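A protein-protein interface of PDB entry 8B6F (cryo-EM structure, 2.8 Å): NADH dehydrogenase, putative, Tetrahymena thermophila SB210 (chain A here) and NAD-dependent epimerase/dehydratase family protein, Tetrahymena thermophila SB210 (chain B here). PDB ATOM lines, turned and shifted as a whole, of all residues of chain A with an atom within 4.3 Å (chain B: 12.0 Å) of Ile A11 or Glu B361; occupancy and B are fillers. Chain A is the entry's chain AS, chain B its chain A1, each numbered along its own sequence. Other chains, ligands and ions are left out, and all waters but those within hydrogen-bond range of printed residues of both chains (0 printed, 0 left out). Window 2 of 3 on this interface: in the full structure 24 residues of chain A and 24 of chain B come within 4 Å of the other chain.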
ATOM      1  N   ASN A   9      34.179  25.874  -6.711  1.00  0.00           N
ATOM      2  CA  ASN A   9      33.608  25.055  -7.769  1.00  0.00           C
ATOM      3  C   ASN A   9      32.524  25.789  -8.548  1.00  0.00           C
ATOM      4  O   ASN A   9      31.731  25.150  -9.247  1.00  0.00           O
ATOM      5  CB  ASN A   9      33.051  23.758  -7.180  1.00  0.00           C
ATOM      6  CG  ASN A   9      32.739  22.722  -8.238  1.00  0.00           C
ATOM      7  OD1 ASN A   9      33.278  22.764  -9.342  1.00  0.00           O
ATOM      8  ND2 ASN A   9      31.865  21.782  -7.907  1.00  0.00           N
ATOM      9  N   THR A  10      32.468  27.111  -8.435  1.00  0.00           N
ATOM     10  CA  THR A  10      31.456  27.887  -9.134  1.00  0.00           C
ATOM     11  C   THR A  10      31.783  27.993 -10.619  1.00  0.00           C
ATOM     12  O   THR A  10      32.940  27.885 -11.034  1.00  0.00           O
ATOM     13  CB  THR A  10      31.355  29.289  -8.533  1.00  0.00           C
ATOM     14  OG1 THR A  10      32.613  29.965  -8.667  1.00  0.00           O
ATOM     15  CG2 THR A  10      30.982  29.222  -7.063  1.00  0.00           C
ATOM     16  N   ILE A  11      30.745  28.199 -11.424  1.00  0.00           N
ATOM     17  CA  ILE A  11      30.908  28.437 -12.856  1.00  0.00           C
ATOM     18  C   ILE A  11      31.271  29.905 -13.047  1.00  0.00           C
ATOM     19  O   ILE A  11      30.517  30.782 -12.602  1.00  0.00           O
ATOM     20  CB  ILE A  11      29.635  28.072 -13.636  1.00  0.00           C
ATOM     21  CG1 ILE A  11      29.278  26.601 -13.404  1.00  0.00           C
ATOM     22  CG2 ILE A  11      29.830  28.351 -15.121  1.00  0.00           C
ATOM     23  CD1 ILE A  11      27.985  26.161 -14.065  1.00  0.00           C
ATOM     24  N   PRO A  12      32.393  30.230 -13.691  1.00  0.00           N
ATOM     25  CA  PRO A  12      32.741  31.645 -13.875  1.00  0.00           C
ATOM     26  C   PRO A  12      31.661  32.392 -14.641  1.00  0.00           C
ATOM     27  O   PRO A  12      31.048  31.858 -15.567  1.00  0.00           O
ATOM     28  CB  PRO A  12      34.053  31.590 -14.666  1.00  0.00           C
ATOM     29  CG  PRO A  12      34.614  30.251 -14.384  1.00  0.00           C
ATOM     30  CD  PRO A  12      33.438  29.340 -14.221  1.00  0.00           C
ATOM     31  N   ALA A  13      31.431  33.644 -14.243  1.00  0.00           N
ATOM     32  CA  ALA A  13      30.432  34.465 -14.913  1.00  0.00           C
ATOM     33  C   ALA A  13      30.917  35.015 -16.244  1.00  0.00           C
ATOM     34  O   ALA A  13      30.096  35.466 -17.048  1.00  0.00           O
ATOM     35  CB  ALA A  13      30.012  35.623 -14.009  1.00  0.00           C
ATOM     36  N   ARG A  32      24.214  23.461 -10.418  1.00  0.00           N
ATOM     37  CA  ARG A  32      25.333  22.535 -10.337  1.00  0.00           C
ATOM     38  C   ARG A  32      26.658  23.278 -10.473  1.00  0.00           C
ATOM     39  O   ARG A  32      26.746  24.330 -11.111  1.00  0.00           O
ATOM     40  CB  ARG A  32      25.224  21.457 -11.415  1.00  0.00           C
ATOM     41  CG  ARG A  32      25.072  21.988 -12.829  1.00  0.00           C
ATOM     42  CD  ARG A  32      25.361  20.897 -13.848  1.00  0.00           C
ATOM     43  NE  ARG A  32      24.946  21.279 -15.191  1.00  0.00           N
ATOM     44  CZ  ARG A  32      23.778  20.969 -15.739  1.00  0.00           C
ATOM     45  NH1 ARG A  32      22.872  20.257 -15.089  1.00  0.00           N
ATOM     46  NH2 ARG A  32      23.511  21.388 -16.972  1.00  0.00           N
ATOM     47  N   GLY A  33      27.696  22.713  -9.868  1.00  0.00           N
ATOM     48  CA  GLY A  33      29.005  23.327  -9.875  1.00  0.00           C
ATOM     49  C   GLY A  33      29.691  23.194 -11.222  1.00  0.00           C
ATOM     50  O   GLY A  33      29.149  22.677 -12.198  1.00  0.00           O
ATOM     51  N   ASN A  34      30.930  23.685 -11.264  1.00  0.00           N
ATOM     52  CA  ASN A  34      31.687  23.686 -12.511  1.00  0.00           C
ATOM     53  C   ASN A  34      32.313  22.323 -12.788  1.00  0.00           C
ATOM     54  O   ASN A  34      32.113  21.747 -13.862  1.00  0.00           O
ATOM     55  CB  ASN A  34      32.763  24.771 -12.461  1.00  0.00           C
ATOM     56  CG  ASN A  34      33.412  25.007 -13.804  1.00  0.00           C
ATOM     57  OD1 ASN A  34      32.873  24.629 -14.841  1.00  0.00           O
ATOM     58  ND2 ASN A  34      34.580  25.636 -13.795  1.00  0.00           N
ATOM     59  N   ASP B 347       8.240  23.769 -24.592  1.00  0.00           N
ATOM     60  CA  ASP B 347       9.453  24.060 -23.834  1.00  0.00           C
ATOM     61  C   ASP B 347      10.655  24.208 -24.759  1.00  0.00           C
ATOM     62  O   ASP B 347      11.458  25.135 -24.610  1.00  0.00           O
ATOM     63  CB  ASP B 347       9.699  22.959 -22.804  1.00  0.00           C
ATOM     64  CG  ASP B 347      10.937  23.211 -21.965  1.00  0.00           C
ATOM     65  OD1 ASP B 347      10.910  24.132 -21.124  1.00  0.00           O
ATOM     66  OD2 ASP B 347      11.938  22.487 -22.150  1.00  0.00           O
ATOM     67  N   ARG B 352      14.669  32.880 -27.080  1.00  0.00           N
ATOM     68  CA  ARG B 352      15.921  33.032 -26.346  1.00  0.00           C
ATOM     69  C   ARG B 352      16.304  34.509 -26.386  1.00  0.00           C
ATOM     70  O   ARG B 352      16.994  34.962 -27.299  1.00  0.00           O
ATOM     71  CB  ARG B 352      17.015  32.147 -26.939  1.00  0.00           C
ATOM     72  CG  ARG B 352      18.369  32.280 -26.254  1.00  0.00           C
ATOM     73  CD  ARG B 352      18.271  31.995 -24.764  1.00  0.00           C
ATOM     74  NE  ARG B 352      19.582  31.917 -24.129  1.00  0.00           N
ATOM     75  CZ  ARG B 352      20.247  32.954 -23.637  1.00  0.00           C
ATOM     76  NH1 ARG B 352      19.762  34.183 -23.700  1.00  0.00           N
ATOM     77  NH2 ARG B 352      21.428  32.751 -23.062  1.00  0.00           N
ATOM     78  N   GLY B 353      15.847  35.253 -25.392  1.00  0.00           N
ATOM     79  CA  GLY B 353      16.180  36.656 -25.235  1.00  0.00           C
ATOM     80  C   GLY B 353      17.253  36.862 -24.188  1.00  0.00           C
ATOM     81  O   GLY B 353      18.219  36.098 -24.100  1.00  0.00           O
ATOM     82  N   VAL B 354      17.080  37.904 -23.382  1.00  0.00           N
ATOM     83  CA  VAL B 354      18.000  38.185 -22.286  1.00  0.00           C
ATOM     84  C   VAL B 354      17.667  37.250 -21.132  1.00  0.00           C
ATOM     85  O   VAL B 354      16.529  37.218 -20.655  1.00  0.00           O
ATOM     86  CB  VAL B 354      17.913  39.655 -21.852  1.00  0.00           C
ATOM     87  CG1 VAL B 354      18.838  39.919 -20.674  1.00  0.00           C
ATOM     88  CG2 VAL B 354      18.257  40.572 -23.014  1.00  0.00           C
ATOM     89  N   GLU B 355      18.658  36.483 -20.687  1.00  0.00           N
ATOM     90  CA  GLU B 355      18.465  35.505 -19.628  1.00  0.00           C
ATOM     91  C   GLU B 355      19.640  35.570 -18.664  1.00  0.00           C
ATOM     92  O   GLU B 355      20.723  36.052 -19.001  1.00  0.00           O
ATOM     93  CB  GLU B 355      18.313  34.089 -20.195  1.00  0.00           C
ATOM     94  CG  GLU B 355      17.084  33.920 -21.071  1.00  0.00           C
ATOM     95  CD  GLU B 355      16.979  32.533 -21.666  1.00  0.00           C
ATOM     96  OE1 GLU B 355      17.988  31.799 -21.640  1.00  0.00           O
ATOM     97  OE2 GLU B 355      15.887  32.175 -22.157  1.00  0.00           O
ATOM     98  N   THR B 356      19.405  35.079 -17.453  1.00  0.00           N
ATOM     99  CA  THR B 356      20.416  35.124 -16.410  1.00  0.00           C
ATOM    100  C   THR B 356      21.548  34.148 -16.717  1.00  0.00           C
ATOM    101  O   THR B 356      21.390  33.181 -17.465  1.00  0.00           O
ATOM    102  CB  THR B 356      19.800  34.792 -15.051  1.00  0.00           C
ATOM    103  OG1 THR B 356      19.237  33.475 -15.084  1.00  0.00           O
ATOM    104  CG2 THR B 356      18.713  35.793 -14.696  1.00  0.00           C
ATOM    105  N   HIS B 357      22.711  34.421 -16.123  1.00  0.00           N
ATOM    106  CA  HIS B 357      23.853  33.529 -16.293  1.00  0.00           C
ATOM    107  C   HIS B 357      23.552  32.146 -15.732  1.00  0.00           C
ATOM    108  O   HIS B 357      23.978  31.132 -16.295  1.00  0.00           O
ATOM    109  CB  HIS B 357      25.090  34.123 -15.623  1.00  0.00           C
ATOM    110  CG  HIS B 357      26.328  33.302 -15.814  1.00  0.00           C
ATOM    111  ND1 HIS B 357      26.789  32.417 -14.863  1.00  0.00           N
ATOM    112  CD2 HIS B 357      27.194  33.224 -16.852  1.00  0.00           C
ATOM    113  CE1 HIS B 357      27.887  31.833 -15.306  1.00  0.00           C
ATOM    114  NE2 HIS B 357      28.155  32.305 -16.510  1.00  0.00           N
ATOM    115  N   ASP B 358      22.824  32.084 -14.617  1.00  0.00           N
ATOM    116  CA  ASP B 358      22.402  30.793 -14.088  1.00  0.00           C
ATOM    117  C   ASP B 358      21.521  30.058 -15.089  1.00  0.00           C
ATOM    118  O   ASP B 358      21.673  28.850 -15.294  1.00  0.00           O
ATOM    119  CB  ASP B 358      21.664  30.983 -12.763  1.00  0.00           C
ATOM    120  CG  ASP B 358      22.528  31.638 -11.704  1.00  0.00           C
ATOM    121  OD1 ASP B 358      23.698  31.955 -12.000  1.00  0.00           O
ATOM    122  OD2 ASP B 358      22.038  31.830 -10.571  1.00  0.00           O
ATOM    123  N   ASN B 359      20.592  30.775 -15.724  1.00  0.00           N
ATOM    124  CA  ASN B 359      19.757  30.171 -16.753  1.00  0.00           C
ATOM    125  C   ASN B 359      20.564  29.740 -17.969  1.00  0.00           C
ATOM    126  O   ASN B 359      20.119  28.861 -18.714  1.00  0.00           O
ATOM    127  CB  ASN B 359      18.664  31.151 -17.178  1.00  0.00           C
ATOM    128  CG  ASN B 359      17.688  30.541 -18.158  1.00  0.00           C
ATOM    129  OD1 ASN B 359      17.951  30.479 -19.357  1.00  0.00           O
ATOM    130  ND2 ASN B 359      16.549  30.086 -17.650  1.00  0.00           N
ATOM    131  N   LEU B 360      21.732  30.344 -18.194  1.00  0.00           N
ATOM    132  CA  LEU B 360      22.575  29.945 -19.314  1.00  0.00           C
ATOM    133  C   LEU B 360      23.088  28.520 -19.170  1.00  0.00           C
ATOM    134  O   LEU B 360      23.477  27.909 -20.172  1.00  0.00           O
ATOM    135  CB  LEU B 360      23.757  30.909 -19.450  1.00  0.00           C
ATOM    136  CG  LEU B 360      24.806  30.569 -20.509  1.00  0.00           C
ATOM    137  CD1 LEU B 360      24.186  30.530 -21.892  1.00  0.00           C
ATOM    138  CD2 LEU B 360      25.945  31.567 -20.464  1.00  0.00           C
ATOM    139  N   GLU B 361      23.105  27.975 -17.952  1.00  0.00           N
ATOM    140  CA  GLU B 361      23.664  26.643 -17.753  1.00  0.00           C
ATOM    141  C   GLU B 361      22.876  25.591 -18.523  1.00  0.00           C
ATOM    142  O   GLU B 361      23.463  24.704 -19.153  1.00  0.00           O
ATOM    143  CB  GLU B 361      23.693  26.305 -16.263  1.00  0.00           C
ATOM    144  CG  GLU B 361      24.201  24.906 -15.957  1.00  0.00           C
ATOM    145  CD  GLU B 361      25.563  24.635 -16.566  1.00  0.00           C
ATOM    146  OE1 GLU B 361      26.330  25.600 -16.762  1.00  0.00           O
ATOM    147  OE2 GLU B 361      25.864  23.459 -16.859  1.00  0.00           O
ATOM    148  N   LYS B 362      21.552  25.668 -18.481  1.00  0.00           N
ATOM    149  CA  LYS B 362      20.708  24.724 -19.204  1.00  0.00           C
ATOM    150  C   LYS B 362      20.938  23.301 -18.709  1.00  0.00           C
ATOM    151  O   LYS B 362      20.262  22.363 -19.132  1.00  0.00           O
ATOM    152  CB  LYS B 362      20.980  24.805 -20.708  1.00  0.00           C
ATOM    153  CG  LYS B 362      19.821  24.340 -21.571  1.00  0.00           C
ATOM    154  CD  LYS B 362      18.726  25.394 -21.640  1.00  0.00           C
ATOM    155  CE  LYS B 362      17.618  24.978 -22.595  1.00  0.00           C
ATOM    156  NZ  LYS B 362      16.545  26.009 -22.687  1.00  0.00           N
ATOM    157  OXT LYS B 362      21.812  23.051 -17.882  1.00  0.00           O
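NE2 of His B357 sits at hydrogen-bond distance from O of Pro A12 (3.1 Å). OE2 of Glu B361 lies within salt-bridge range of NE of Arg A32 (2.9 Å). The chain-end carboxylate of Lys B362 lies within salt-bridge range of the guanidinium group of Arg A32.
Ile A11 touches His B357 (O to CE1, 3.9 Å). Glu B361 touches Ile A11. Ala A13 touches His B357 (CA to NE2, 3.5 Å).
No residue of chain B comes within 4 Å of Thr A10. Of chain B, only His B357 (3.9 Å) and Glu B361 (3.2 Å) come within 4 Å of Ile A11. Pro A12 touches one residue of chain B. Ala A13 touches one residue of chain B. Printed residues of chain A within 4 Å of His B357: Ile A11 (3.9 Å), Pro A12 (3.1 Å) and Ala A13 (3.5 Å). Of chain A, only Ile A11 and Arg A32 come within 4 Å of Glu B361. Printed residues of chain A within 4 Å of Lys B362: Arg A32.
Hydrophobic or aromatic side chains of chain B that line the printed part of chain A: His B357. Along chain B the printed residues that touch a printed residue of chain A span positions 357 to 362. Among the printed residues, 6 pairs touch across the chains.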
